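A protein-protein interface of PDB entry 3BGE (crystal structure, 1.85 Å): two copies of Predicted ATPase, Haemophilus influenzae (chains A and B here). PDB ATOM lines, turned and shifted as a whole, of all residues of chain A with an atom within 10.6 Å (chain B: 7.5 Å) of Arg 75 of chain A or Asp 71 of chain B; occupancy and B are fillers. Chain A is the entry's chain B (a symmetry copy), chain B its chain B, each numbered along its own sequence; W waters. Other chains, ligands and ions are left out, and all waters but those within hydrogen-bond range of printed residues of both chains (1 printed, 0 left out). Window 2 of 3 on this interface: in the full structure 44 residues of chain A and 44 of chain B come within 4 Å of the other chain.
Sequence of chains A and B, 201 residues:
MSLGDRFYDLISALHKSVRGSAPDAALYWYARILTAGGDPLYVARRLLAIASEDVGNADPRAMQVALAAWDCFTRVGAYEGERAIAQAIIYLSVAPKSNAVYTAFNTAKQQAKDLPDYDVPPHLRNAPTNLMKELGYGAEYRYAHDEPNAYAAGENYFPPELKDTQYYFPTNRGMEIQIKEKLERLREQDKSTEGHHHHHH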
ATOM      1  N   LEU A  41      -8.069   0.618 -35.265  1.00  0.00           N
ATOM      2  CA  LEU A  41      -8.989   0.913 -34.151  1.00  0.00           C
ATOM      3  C   LEU A  41      -9.616   2.305 -34.266  1.00  0.00           C
ATOM      4  O   LEU A  41     -10.723   2.534 -33.775  1.00  0.00           O
ATOM      5  CB  LEU A  41      -8.288   0.750 -32.788  1.00  0.00           C
ATOM      6  CG  LEU A  41      -8.023  -0.687 -32.301  1.00  0.00           C
ATOM      7  CD1 LEU A  41      -7.800  -0.631 -30.788  1.00  0.00           C
ATOM      8  CD2 LEU A  41      -9.155  -1.623 -32.628  1.00  0.00           C
ATOM      9  N   LEU A  67     -18.195  -5.021 -32.147  1.00  0.00           N
ATOM     10  CA  LEU A  67     -17.379  -5.278 -30.935  1.00  0.00           C
ATOM     11  C   LEU A  67     -16.600  -6.574 -31.086  1.00  0.00           C
ATOM     12  O   LEU A  67     -15.476  -6.670 -30.649  1.00  0.00           O
ATOM     13  CB  LEU A  67     -18.239  -5.336 -29.646  1.00  0.00           C
ATOM     14  CG  LEU A  67     -18.875  -4.009 -29.222  1.00  0.00           C
ATOM     15  CD1 LEU A  67     -20.058  -4.274 -28.225  1.00  0.00           C
ATOM     16  CD2 LEU A  67     -17.794  -3.073 -28.620  1.00  0.00           C
ATOM     17  N   ALA A  68     -17.209  -7.586 -31.710  1.00  0.00           N
ATOM     18  CA  ALA A  68     -16.528  -8.850 -31.919  1.00  0.00           C
ATOM     19  C   ALA A  68     -15.328  -8.710 -32.870  1.00  0.00           C
ATOM     20  O   ALA A  68     -14.257  -9.274 -32.613  1.00  0.00           O
ATOM     21  CB  ALA A  68     -17.534  -9.968 -32.417  1.00  0.00           C
ATOM     22  N   ALA A  69     -15.472  -7.916 -33.928  1.00  0.00           N
ATOM     23  CA  ALA A  69     -14.315  -7.577 -34.773  1.00  0.00           C
ATOM     24  C   ALA A  69     -13.147  -6.939 -33.981  1.00  0.00           C
ATOM     25  O   ALA A  69     -11.957  -7.334 -34.122  1.00  0.00           O
ATOM     26  CB  ALA A  69     -14.753  -6.661 -35.936  1.00  0.00           C
ATOM     27  N   TRP A  70     -13.492  -5.981 -33.126  1.00  0.00           N
ATOM     28  CA  TRP A  70     -12.508  -5.365 -32.238  1.00  0.00           C
ATOM     29  C   TRP A  70     -11.861  -6.393 -31.297  1.00  0.00           C
ATOM     30  O   TRP A  70     -10.634  -6.362 -31.067  1.00  0.00           O
ATOM     31  CB  TRP A  70     -13.172  -4.236 -31.441  1.00  0.00           C
ATOM     32  CG  TRP A  70     -12.256  -3.357 -30.625  1.00  0.00           C
ATOM     33  CD1 TRP A  70     -11.116  -3.719 -29.950  1.00  0.00           C
ATOM     34  CD2 TRP A  70     -12.435  -1.960 -30.384  1.00  0.00           C
ATOM     35  NE1 TRP A  70     -10.568  -2.616 -29.311  1.00  0.00           N
ATOM     36  CE2 TRP A  70     -11.356  -1.527 -29.573  1.00  0.00           C
ATOM     37  CE3 TRP A  70     -13.392  -1.018 -30.810  1.00  0.00           C
ATOM     38  CZ2 TRP A  70     -11.223  -0.206 -29.152  1.00  0.00           C
ATOM     39  CZ3 TRP A  70     -13.263   0.292 -30.390  1.00  0.00           C
ATOM     40  CH2 TRP A  70     -12.178   0.688 -29.560  1.00  0.00           C
ATOM     41  N   ASP A  71     -12.661  -7.307 -30.752  1.00  0.00           N
ATOM     42  CA  ASP A  71     -12.115  -8.380 -29.912  1.00  0.00           C
ATOM     43  C   ASP A  71     -11.117  -9.255 -30.669  1.00  0.00           C
ATOM     44  O   ASP A  71     -10.153  -9.733 -30.102  1.00  0.00           O
ATOM     45  CB  ASP A  71     -13.248  -9.238 -29.354  1.00  0.00           C
ATOM     46  CG  ASP A  71     -13.983  -8.540 -28.220  1.00  0.00           C
ATOM     47  OD1 ASP A  71     -13.471  -7.512 -27.718  1.00  0.00           O
ATOM     48  OD2 ASP A  71     -15.085  -8.992 -27.848  1.00  0.00           O
ATOM     49  N   CYS A  72     -11.365  -9.499 -31.949  1.00  0.00           N
ATOM     50  CA  CYS A  72     -10.410 -10.246 -32.765  1.00  0.00           C
ATOM     51  C   CYS A  72      -9.068  -9.539 -32.860  1.00  0.00           C
ATOM     52  O   CYS A  72      -8.022 -10.164 -32.761  1.00  0.00           O
ATOM     53  CB  CYS A  72     -10.986 -10.498 -34.165  1.00  0.00           C
ATOM     54  SG  CYS A  72     -12.235 -11.784 -34.121  1.00  0.00           S
ATOM     55  N   PHE A  73      -9.106  -8.226 -33.083  1.00  0.00           N
ATOM     56  CA  PHE A  73      -7.910  -7.397 -33.136  1.00  0.00           C
ATOM     57  C   PHE A  73      -7.140  -7.509 -31.817  1.00  0.00           C
ATOM     58  O   PHE A  73      -5.905  -7.705 -31.798  1.00  0.00           O
ATOM     59  CB  PHE A  73      -8.329  -5.944 -33.392  1.00  0.00           C
ATOM     60  CG  PHE A  73      -7.176  -4.954 -33.365  1.00  0.00           C
ATOM     61  CD1 PHE A  73      -6.542  -4.567 -34.546  1.00  0.00           C
ATOM     62  CD2 PHE A  73      -6.770  -4.382 -32.170  1.00  0.00           C
ATOM     63  CE1 PHE A  73      -5.461  -3.649 -34.519  1.00  0.00           C
ATOM     64  CE2 PHE A  73      -5.743  -3.461 -32.148  1.00  0.00           C
ATOM     65  CZ  PHE A  73      -5.091  -3.090 -33.333  1.00  0.00           C
ATOM     66  N   THR A  74      -7.882  -7.406 -30.718  1.00  0.00           N
ATOM     67  CA  THR A  74      -7.314  -7.404 -29.363  1.00  0.00           C
ATOM     68  C   THR A  74      -6.651  -8.716 -28.933  1.00  0.00           C
ATOM     69  O   THR A  74      -5.680  -8.725 -28.161  1.00  0.00           O
ATOM     70  CB  THR A  74      -8.393  -7.072 -28.334  1.00  0.00           C
ATOM     71  OG1 THR A  74      -8.751  -5.691 -28.444  1.00  0.00           O
ATOM     72  CG2 THR A  74      -7.864  -7.313 -26.962  1.00  0.00           C
ATOM     73  N   ARG A  75      -7.187  -9.814 -29.438  1.00  0.00           N
ATOM     74  CA  ARG A  75      -6.735 -11.167 -29.094  1.00  0.00           C
ATOM     75  C   ARG A  75      -5.794 -11.827 -30.075  1.00  0.00           C
ATOM     76  O   ARG A  75      -4.881 -12.532 -29.664  1.00  0.00           O
ATOM     77  CB  ARG A  75      -7.973 -12.076 -28.965  1.00  0.00           C
ATOM     78  CG  ARG A  75      -8.779 -11.723 -27.762  1.00  0.00           C
ATOM     79  CD  ARG A  75      -9.766 -12.794 -27.401  1.00  0.00           C
ATOM     80  NE  ARG A  75     -10.864 -12.147 -26.726  1.00  0.00           N
ATOM     81  CZ  ARG A  75     -11.844 -12.758 -26.070  1.00  0.00           C
ATOM     82  NH1 ARG A  75     -11.889 -14.078 -25.959  1.00  0.00           N
ATOM     83  NH2 ARG A  75     -12.792 -12.019 -25.523  1.00  0.00           N
ATOM     84  N   VAL A  76      -6.037 -11.658 -31.372  1.00  0.00           N
ATOM     85  CA  VAL A  76      -5.229 -12.324 -32.397  1.00  0.00           C
ATOM     86  C   VAL A  76      -4.120 -11.369 -32.849  1.00  0.00           C
ATOM     87  O   VAL A  76      -2.919 -11.720 -32.772  1.00  0.00           O
ATOM     88  CB  VAL A  76      -6.099 -12.794 -33.581  1.00  0.00           C
ATOM     89  CG1 VAL A  76      -5.286 -13.602 -34.565  1.00  0.00           C
ATOM     90  CG2 VAL A  76      -7.300 -13.639 -33.050  1.00  0.00           C
ATOM     91  N   GLY A  77      -4.521 -10.161 -33.279  1.00  0.00           N
ATOM     92  CA  GLY A  77      -3.580  -9.120 -33.645  1.00  0.00           C
ATOM     93  C   GLY A  77      -4.040  -8.218 -34.781  1.00  0.00           C
ATOM     94  O   GLY A  77      -5.202  -8.238 -35.206  1.00  0.00           O
ATOM     95  N   ALA A  78      -3.094  -7.464 -35.310  1.00  0.00           N
ATOM     96  CA  ALA A  78      -3.419  -6.359 -36.192  1.00  0.00           C
ATOM     97  C   ALA A  78      -3.953  -6.856 -37.540  1.00  0.00           C
ATOM     98  O   ALA A  78      -4.914  -6.299 -38.088  1.00  0.00           O
ATOM     99  CB  ALA A  78      -2.147  -5.430 -36.355  1.00  0.00           C
ATOM    100  N   TYR A  79      -3.365  -7.936 -38.051  1.00  0.00           N
ATOM    101  CA  TYR A  79      -3.651  -8.355 -39.395  1.00  0.00           C
ATOM    102  C   TYR A  79      -4.948  -9.113 -39.497  1.00  0.00           C
ATOM    103  O   TYR A  79      -5.750  -8.831 -40.383  1.00  0.00           O
ATOM    104  CB  TYR A  79      -2.483  -9.121 -40.015  1.00  0.00           C
ATOM    105  CG  TYR A  79      -1.365  -8.162 -40.263  1.00  0.00           C
ATOM    106  CD1 TYR A  79      -1.534  -7.111 -41.156  1.00  0.00           C
ATOM    107  CD2 TYR A  79      -0.158  -8.287 -39.598  1.00  0.00           C
ATOM    108  CE1 TYR A  79      -0.548  -6.200 -41.375  1.00  0.00           C
ATOM    109  CE2 TYR A  79       0.852  -7.391 -39.819  1.00  0.00           C
ATOM    110  CZ  TYR A  79       0.651  -6.343 -40.715  1.00  0.00           C
ATOM    111  OH  TYR A  79       1.644  -5.435 -40.961  1.00  0.00           O
ATOM    112  N   GLU A  80      -5.159 -10.061 -38.599  1.00  0.00           N
ATOM    113  CA  GLU A  80      -6.485 -10.709 -38.503  1.00  0.00           C
ATOM    114  C   GLU A  80      -7.547  -9.698 -38.016  1.00  0.00           C
ATOM    115  O   GLU A  80      -8.711  -9.763 -38.427  1.00  0.00           O
ATOM    116  CB  GLU A  80      -6.408 -11.918 -37.552  1.00  0.00           C
ATOM    117  CG  GLU A  80      -7.738 -12.341 -36.977  1.00  0.00           C
ATOM    118  CD  GLU A  80      -8.752 -12.792 -38.056  1.00  0.00           C
ATOM    119  OE1 GLU A  80      -8.326 -13.251 -39.136  1.00  0.00           O
ATOM    120  OE2 GLU A  80      -9.976 -12.694 -37.798  1.00  0.00           O
ATOM    121  N   GLY A  81      -7.144  -8.762 -37.147  1.00  0.00           N
ATOM    122  CA  GLY A  81      -8.005  -7.656 -36.727  1.00  0.00           C
ATOM    123  C   GLY A  81      -8.545  -6.877 -37.910  1.00  0.00           C
ATOM    124  O   GLY A  81      -9.754  -6.665 -38.017  1.00  0.00           O
ATOM    125  N   GLU A  82      -7.647  -6.474 -38.812  1.00  0.00           N
ATOM    126  CA  GLU A  82      -8.008  -5.762 -40.052  1.00  0.00           C
ATOM    127  C   GLU A  82      -9.092  -6.478 -40.841  1.00  0.00           C
ATOM    128  O   GLU A  82     -10.069  -5.863 -41.275  1.00  0.00           O
ATOM    129  CB  GLU A  82      -6.775  -5.635 -40.953  1.00  0.00           C
ATOM    130  CG  GLU A  82      -6.047  -4.365 -40.765  1.00  0.00           C
ATOM    131  CD  GLU A  82      -4.844  -4.259 -41.694  1.00  0.00           C
ATOM    132  OE1 GLU A  82      -4.730  -5.023 -42.698  1.00  0.00           O
ATOM    133  OE2 GLU A  82      -3.989  -3.422 -41.374  1.00  0.00           O
ATOM    134  N   ALA A  84     -11.184  -8.904 -39.657  1.00  0.00           N
ATOM    135  CA  ALA A  84     -12.456  -8.910 -38.926  1.00  0.00           C
ATOM    136  C   ALA A  84     -13.211  -7.570 -39.035  1.00  0.00           C
ATOM    137  O   ALA A  84     -14.458  -7.543 -39.134  1.00  0.00           O
ATOM    138  CB  ALA A  84     -12.225  -9.275 -37.416  1.00  0.00           C
ATOM    139  N   ILE A  85     -12.481  -6.465 -38.959  1.00  0.00           N
ATOM    140  CA  ILE A  85     -13.072  -5.127 -39.101  1.00  0.00           C
ATOM    141  C   ILE A  85     -13.622  -4.935 -40.532  1.00  0.00           C
ATOM    142  O   ILE A  85     -14.679  -4.314 -40.723  1.00  0.00           O
ATOM    143  CB  ILE A  85     -12.047  -4.028 -38.709  1.00  0.00           C
ATOM    144  CG1 ILE A  85     -11.768  -4.108 -37.213  1.00  0.00           C
ATOM    145  CG2 ILE A  85     -12.540  -2.600 -39.065  1.00  0.00           C
ATOM    146  CD1 ILE A  85     -10.490  -3.363 -36.807  1.00  0.00           C
ATOM    147  N   LEU B  41      -4.988 -22.141 -26.943  1.00  0.00           N
ATOM    148  CA  LEU B  41      -5.175 -20.773 -27.460  1.00  0.00           C
ATOM    149  C   LEU B  41      -4.469 -20.554 -28.801  1.00  0.00           C
ATOM    150  O   LEU B  41      -4.896 -19.723 -29.603  1.00  0.00           O
ATOM    151  CB  LEU B  41      -4.715 -19.719 -26.433  1.00  0.00           C
ATOM    152  CG  LEU B  41      -5.630 -19.476 -25.218  1.00  0.00           C
ATOM    153  CD1 LEU B  41      -5.268 -18.111 -24.629  1.00  0.00           C
ATOM    154  CD2 LEU B  41      -7.090 -19.520 -25.579  1.00  0.00           C
ATOM    155  N   ARG B  45      -6.758 -18.918 -31.593  1.00  0.00           N
ATOM    156  CA  ARG B  45      -6.427 -17.789 -32.435  1.00  0.00           C
ATOM    157  C   ARG B  45      -6.616 -18.158 -33.899  1.00  0.00           C
ATOM    158  O   ARG B  45      -7.072 -17.331 -34.694  1.00  0.00           O
ATOM    159  CB  ARG B  45      -4.970 -17.395 -32.215  1.00  0.00           C
ATOM    160  CG  ARG B  45      -4.811 -16.551 -30.997  1.00  0.00           C
ATOM    161  CD  ARG B  45      -3.341 -16.047 -30.805  1.00  0.00           C
ATOM    162  NE  ARG B  45      -2.413 -17.107 -30.397  1.00  0.00           N
ATOM    163  CZ  ARG B  45      -2.196 -17.501 -29.136  1.00  0.00           C
ATOM    164  NH1 ARG B  45      -2.847 -16.958 -28.099  1.00  0.00           N
ATOM    165  NH2 ARG B  45      -1.343 -18.491 -28.916  1.00  0.00           N
ATOM    166  N   LEU B  48     -10.352 -18.121 -34.882  1.00  0.00           N
ATOM    167  CA  LEU B  48     -10.817 -16.789 -35.199  1.00  0.00           C
ATOM    168  C   LEU B  48     -10.414 -16.452 -36.629  1.00  0.00           C
ATOM    169  O   LEU B  48     -11.192 -15.846 -37.359  1.00  0.00           O
ATOM    170  CB  LEU B  48     -10.241 -15.768 -34.190  1.00  0.00           C
ATOM    171  CG  LEU B  48     -10.923 -15.806 -32.805  1.00  0.00           C
ATOM    172  CD1 LEU B  48     -10.257 -14.934 -31.760  1.00  0.00           C
ATOM    173  CD2 LEU B  48     -12.346 -15.333 -32.977  1.00  0.00           C
ATOM    174  N   GLN B  64     -18.452 -14.670 -32.850  1.00  0.00           N
ATOM    175  CA  GLN B  64     -18.869 -14.669 -31.454  1.00  0.00           C
ATOM    176  C   GLN B  64     -18.797 -16.060 -30.811  1.00  0.00           C
ATOM    177  O   GLN B  64     -18.525 -16.168 -29.635  1.00  0.00           O
ATOM    178  CB  GLN B  64     -20.256 -14.047 -31.277  1.00  0.00           C
ATOM    179  CG  GLN B  64     -20.258 -12.544 -31.611  1.00  0.00           C
ATOM    180  CD  GLN B  64     -21.619 -12.035 -32.078  1.00  0.00           C
ATOM    181  OE1 GLN B  64     -22.652 -12.404 -31.522  1.00  0.00           O
ATOM    182  NE2 GLN B  64     -21.617 -11.206 -33.111  1.00  0.00           N
ATOM    183  N   VAL B  65     -19.053 -17.122 -31.562  1.00  0.00           N
ATOM    184  CA  VAL B  65     -19.007 -18.468 -30.958  1.00  0.00           C
ATOM    185  C   VAL B  65     -17.565 -18.762 -30.592  1.00  0.00           C
ATOM    186  O   VAL B  65     -17.269 -19.243 -29.498  1.00  0.00           O
ATOM    187  CB  VAL B  65     -19.538 -19.543 -31.945  1.00  0.00           C
ATOM    188  CG1 VAL B  65     -19.299 -20.917 -31.406  1.00  0.00           C
ATOM    189  CG2 VAL B  65     -21.034 -19.300 -32.219  1.00  0.00           C
ATOM    190  N   ALA B  66     -16.652 -18.442 -31.500  1.00  0.00           N
ATOM    191  CA  ALA B  66     -15.250 -18.689 -31.243  1.00  0.00           C
ATOM    192  C   ALA B  66     -14.735 -17.823 -30.083  1.00  0.00           C
ATOM    193  O   ALA B  66     -13.976 -18.310 -29.243  1.00  0.00           O
ATOM    194  CB  ALA B  66     -14.432 -18.461 -32.520  1.00  0.00           C
ATOM    195  N   LEU B  67     -15.161 -16.557 -30.003  1.00  0.00           N
ATOM    196  CA  LEU B  67     -14.725 -15.690 -28.882  1.00  0.00           C
ATOM    197  C   LEU B  67     -15.296 -16.199 -27.568  1.00  0.00           C
ATOM    198  O   LEU B  67     -14.641 -16.146 -26.551  1.00  0.00           O
ATOM    199  CB  LEU B  67     -15.134 -14.209 -29.086  1.00  0.00           C
ATOM    200  CG  LEU B  67     -14.419 -13.485 -30.230  1.00  0.00           C
ATOM    201  CD1 LEU B  67     -15.221 -12.197 -30.636  1.00  0.00           C
ATOM    202  CD2 LEU B  67     -12.957 -13.166 -29.824  1.00  0.00           C
ATOM    203  N   ALA B  68     -16.537 -16.693 -27.589  1.00  0.00           N
ATOM    204  CA  ALA B  68     -17.148 -17.223 -26.385  1.00  0.00           C
ATOM    205  C   ALA B  68     -16.430 -18.484 -25.877  1.00  0.00           C
ATOM    206  O   ALA B  68     -16.198 -18.629 -24.671  1.00  0.00           O
ATOM    207  CB  ALA B  68     -18.697 -17.484 -26.595  1.00  0.00           C
ATOM    208  N   ALA B  69     -16.019 -19.364 -26.786  1.00  0.00           N
ATOM    209  CA  ALA B  69     -15.156 -20.492 -26.399  1.00  0.00           C
ATOM    210  C   ALA B  69     -13.853 -20.049 -25.689  1.00  0.00           C
ATOM    211  O   ALA B  69     -13.464 -20.592 -24.618  1.00  0.00           O
ATOM    212  CB  ALA B  69     -14.839 -21.369 -27.629  1.00  0.00           C
ATOM    213  N   TRP B  70     -13.202 -19.043 -26.265  1.00  0.00           N
ATOM    214  CA  TRP B  70     -12.015 -18.454 -25.648  1.00  0.00           C
ATOM    215  C   TRP B  70     -12.322 -17.864 -24.263  1.00  0.00           C
ATOM    216  O   TRP B  70     -11.530 -18.027 -23.312  1.00  0.00           O
ATOM    217  CB  TRP B  70     -11.429 -17.387 -26.579  1.00  0.00           C
ATOM    218  CG  TRP B  70     -10.084 -16.820 -26.194  1.00  0.00           C
ATOM    219  CD1 TRP B  70      -9.601 -16.572 -24.932  1.00  0.00           C
ATOM    220  CD2 TRP B  70      -9.062 -16.404 -27.101  1.00  0.00           C
ATOM    221  NE1 TRP B  70      -8.323 -16.036 -25.007  1.00  0.00           N
ATOM    222  CE2 TRP B  70      -7.972 -15.934 -26.326  1.00  0.00           C
ATOM    223  CE3 TRP B  70      -8.948 -16.419 -28.505  1.00  0.00           C
ATOM    224  CZ2 TRP B  70      -6.799 -15.454 -26.904  1.00  0.00           C
ATOM    225  CZ3 TRP B  70      -7.785 -15.940 -29.079  1.00  0.00           C
ATOM    226  CH2 TRP B  70      -6.719 -15.457 -28.272  1.00  0.00           C
ATOM    227  N   ASP B  71     -13.460 -17.184 -24.129  1.00  0.00           N
ATOM    228  CA  ASP B  71     -13.875 -16.662 -22.821  1.00  0.00           C
ATOM    229  C   ASP B  71     -14.055 -17.772 -21.788  1.00  0.00           C
ATOM    230  O   ASP B  71     -13.782 -17.581 -20.617  1.00  0.00           O
ATOM    231  CB  ASP B  71     -15.167 -15.861 -22.964  1.00  0.00           C
ATOM    232  CG  ASP B  71     -14.922 -14.493 -23.583  1.00  0.00           C
ATOM    233  OD1 ASP B  71     -13.742 -14.083 -23.679  1.00  0.00           O
ATOM    234  OD2 ASP B  71     -15.897 -13.840 -24.004  1.00  0.00           O
ATOM    235  N   CYS B  72     -14.552 -18.927 -22.210  1.00  0.00           N
ATOM    236  CA  CYS B  72     -14.663 -20.066 -21.302  1.00  0.00           C
ATOM    237  C   CYS B  72     -13.308 -20.510 -20.775  1.00  0.00           C
ATOM    238  O   CYS B  72     -13.159 -20.803 -19.597  1.00  0.00           O
ATOM    239  CB  CYS B  72     -15.379 -21.234 -21.996  1.00  0.00           C
ATOM    240  SG  CYS B  72     -17.141 -20.922 -22.119  1.00  0.00           S
ATOM    241  N   PHE B  73     -12.323 -20.585 -21.669  1.00  0.00           N
ATOM    242  CA  PHE B  73     -10.955 -20.932 -21.311  1.00  0.00           C
ATOM    243  C   PHE B  73     -10.419 -19.936 -20.278  1.00  0.00           C
ATOM    244  O   PHE B  73      -9.827 -20.323 -19.245  1.00  0.00           O
ATOM    245  CB  PHE B  73     -10.092 -20.906 -22.578  1.00  0.00           C
ATOM    246  CG  PHE B  73      -8.614 -21.148 -22.325  1.00  0.00           C
ATOM    247  CD1 PHE B  73      -8.069 -22.426 -22.453  1.00  0.00           C
ATOM    248  CD2 PHE B  73      -7.773 -20.092 -22.012  1.00  0.00           C
ATOM    249  CE1 PHE B  73      -6.690 -22.653 -22.209  1.00  0.00           C
ATOM    250  CE2 PHE B  73      -6.425 -20.305 -21.812  1.00  0.00           C
ATOM    251  CZ  PHE B  73      -5.883 -21.595 -21.918  1.00  0.00           C
ATOM    252  N   THR B  74     -10.652 -18.656 -20.551  1.00  0.00           N
ATOM    253  CA  THR B  74     -10.144 -17.553 -19.725  1.00  0.00           C
ATOM    254  C   THR B  74     -10.727 -17.477 -18.311  1.00  0.00           C
ATOM    255  O   THR B  74     -10.055 -17.051 -17.358  1.00  0.00           O
ATOM    256  CB  THR B  74     -10.409 -16.212 -20.406  1.00  0.00           C
ATOM    257  OG1 THR B  74      -9.549 -16.074 -21.541  1.00  0.00           O
ATOM    258  CG2 THR B  74     -10.113 -15.103 -19.455  1.00  0.00           C
ATOM    259  N   ARG B  75     -11.978 -17.889 -18.190  1.00  0.00           N
ATOM    260  CA  ARG B  75     -12.731 -17.833 -16.931  1.00  0.00           C
ATOM    261  C   ARG B  75     -12.803 -19.117 -16.137  1.00  0.00           C
ATOM    262  O   ARG B  75     -12.758 -19.079 -14.914  1.00  0.00           O
ATOM    263  CB  ARG B  75     -14.178 -17.409 -17.249  1.00  0.00           C
ATOM    264  CG  ARG B  75     -14.240 -15.987 -17.690  1.00  0.00           C
ATOM    265  CD  ARG B  75     -15.636 -15.438 -17.655  1.00  0.00           C
ATOM    266  NE  ARG B  75     -15.706 -14.396 -18.648  1.00  0.00           N
ATOM    267  CZ  ARG B  75     -16.699 -13.526 -18.798  1.00  0.00           C
ATOM    268  NH1 ARG B  75     -17.753 -13.531 -17.995  1.00  0.00           N
ATOM    269  NH2 ARG B  75     -16.621 -12.643 -19.776  1.00  0.00           N
ATOM    270  N   VAL B  76     -12.973 -20.250 -16.812  1.00  0.00           N
ATOM    271  CA  VAL B  76     -13.135 -21.535 -16.124  1.00  0.00           C
ATOM    272  C   VAL B  76     -11.768 -22.219 -16.028  1.00  0.00           C
ATOM    273  O   VAL B  76     -11.311 -22.554 -14.910  1.00  0.00           O
ATOM    274  CB  VAL B  76     -14.174 -22.426 -16.837  1.00  0.00           C
ATOM    275  CG1 VAL B  76     -14.439 -23.686 -16.047  1.00  0.00           C
ATOM    276  CG2 VAL B  76     -15.499 -21.627 -17.043  1.00  0.00           C
ATOM    277  N   GLY B  77     -11.109 -22.386 -17.186  1.00  0.00           N
ATOM    278  CA  GLY B  77      -9.765 -22.929 -17.239  1.00  0.00           C
ATOM    279  C   GLY B  77      -9.468 -23.774 -18.470  1.00  0.00           C
ATOM    280  O   GLY B  77     -10.237 -23.814 -19.439  1.00  0.00           O
ATOM    281  N   GLY B  81     -12.055 -25.091 -21.135  1.00  0.00           N
ATOM    282  CA  GLY B  81     -11.651 -24.320 -22.311  1.00  0.00           C
ATOM    283  C   GLY B  81     -11.505 -25.196 -23.541  1.00  0.00           C
ATOM    284  O   GLY B  81     -12.081 -24.899 -24.589  1.00  0.00           O
ATOM    285  N   ALA B  84     -14.906 -26.213 -24.775  1.00  0.00           N
ATOM    286  CA  ALA B  84     -15.589 -25.125 -25.484  1.00  0.00           C
ATOM    287  C   ALA B  84     -15.001 -24.866 -26.886  1.00  0.00           C
ATOM    288  O   ALA B  84     -15.744 -24.566 -27.847  1.00  0.00           O
ATOM    289  CB  ALA B  84     -15.555 -23.803 -24.635  1.00  0.00           C
ATOM    290  N   ILE B  85     -13.680 -24.918 -26.998  1.00  0.00           N
ATOM    291  CA  ILE B  85     -12.999 -24.742 -28.287  1.00  0.00           C
ATOM    292  C   ILE B  85     -13.352 -25.905 -29.242  1.00  0.00           C
ATOM    293  O   ILE B  85     -13.523 -25.696 -30.453  1.00  0.00           O
ATOM    294  CB  ILE B  85     -11.466 -24.589 -28.085  1.00  0.00           C
ATOM    295  CG1 ILE B  85     -11.180 -23.270 -27.377  1.00  0.00           C
ATOM    296  CG2 ILE B  85     -10.680 -24.637 -29.422  1.00  0.00           C
ATOM    297  CD1 ILE B  85      -9.773 -23.216 -26.769  1.00  0.00           C
HETATM  298  O   HOH W   1      -3.453 -14.000 -27.937  1.00  0.00           O
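Of the 19 printed residues of chain A, 6 touch a printed residue of chain B.
Hydrophobic or aromatic side chains of chain A that line the printed part of chain B: Ala 68 and Val 76.
Of the 20 printed residues of chain B, 5 touch a printed residue of chain A.
Printed residues of chain B that touch a printed residue of chain A: Leu 48, Gln 64, Leu 67, Trp 70 and Asp 71.
Hydrophobic or aromatic side chains of chain B that line the printed part of chain A: Leu 48, Leu 67 and Trp 70.
Among the printed residues, pairs that only touch across the chains: Ala 68 of chain A with Gln 64 of chain B, Ala 68 of chain A with Leu 67 of chain B, Asp 71 of chain A with Leu 67 of chain B, Cys 72 of chain A with Leu 48 of chain B, Arg 75 of chain A with Trp 70 of chain B and Val 76 of chain A with Leu 48 of chain B.
Water W1 bridges the backbone carbonyl oxygen of Arg 75 of chain A and the guanidinium group of Arg 45 of chain B.
The backbone carbonyl oxygen of Trp 70 of chain B sits at hydrogen-bond distance from the side-chain hydroxyl of Thr 74 of chain B (3.3 Å).
The side-chain sulfur (SG) of Cys 72 of chain A is in hydrogen-bond range of the backbone carbonyl oxygen (O) of Ala 68 of chain A (3.6 Å).
The side-chain carboxylate (OD1) of Asp 71 of chain B is in salt-bridge range of the guanidinium group (NH2) of Arg 75 of chain A.
The guanidinium group of Arg 75 of chain A sits at hydrogen-bond distance from the backbone carbonyl oxygen of Leu 67 of chain B, at 3.5 Å.
The side-chain carboxylate of Glu 80 of chain A lies close to the backbone carbonyl oxygen of Leu 48 of chain B, at 3.4 Å.
Ala 68 of chain A touches Leu 67 of chain B, but with the chains exchanged Leu 67 of chain A does not touch Ala 68 of chain B (10.5 Å).
Arg 75 of chain A touches Leu 67 of chain B, but with the chains exchanged Leu 67 of chain A does not touch Arg 75 of chain B (12.4 Å).
Arg 75 of chain A touches Trp 70 of chain B, but with the chains exchanged Trp 70 of chain A does not touch Arg 75 of chain B (13.9 Å).
Positions printed for both chains: 41, 67, 68, 69, 70, 71, 72, 73, 74, 75, 76, 77, 81, 84 and 85.
Of the 9 pairs that touch across the chains among the printed residues, none has its exchanged pair printed and touching as well.
Printed residues of chain B within 4 Å of Ala 68 of chain A: Gln 64 and Leu 67.
Printed residues of chain B within 4 Å of Arg 75 of chain A: Leu 67 (3.5 Å), Trp 70 (3.3 Å) and Asp 71 (2.9 Å).
Gly 77 of chain A touches none of the printed residues of chain B.
Of the printed residues of chain B, Glu 80 of chain A touches Leu 48 (3.4 Å).
Of the printed residues of chain A, Leu 48 of chain B touches Cys 72 (3.7 Å), Val 76 (3.5 Å) and Glu 80 (3.4 Å).
Of the printed residues of chain A, Gln 64 of chain B touches Ala 68 (3.8 Å).
Ala 66 of chain B touches none of the printed residues of chain A.
Leu 67 of chain B touches three residues of chain A.
No residue of chain A comes within 4 Å of Ala 68 of chain B.
No residue of chain A comes within 4 Å of Ala 69 of chain B.
Printed residues of chain A within 4 Å of Trp 70 of chain B: Arg 75 (3.3 Å).
Asp 71 of chain B touches just one residue of chain A: Arg 75.
No residue of chain A comes within 4 Å of Thr 74 of chain B.
No residue of chain A comes within 4 Å of Arg 75 of chain B.
The nearest printed residue of chain B that does not touch Asp 71 of chain A is Leu 48 of chain B (5.5 Å).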
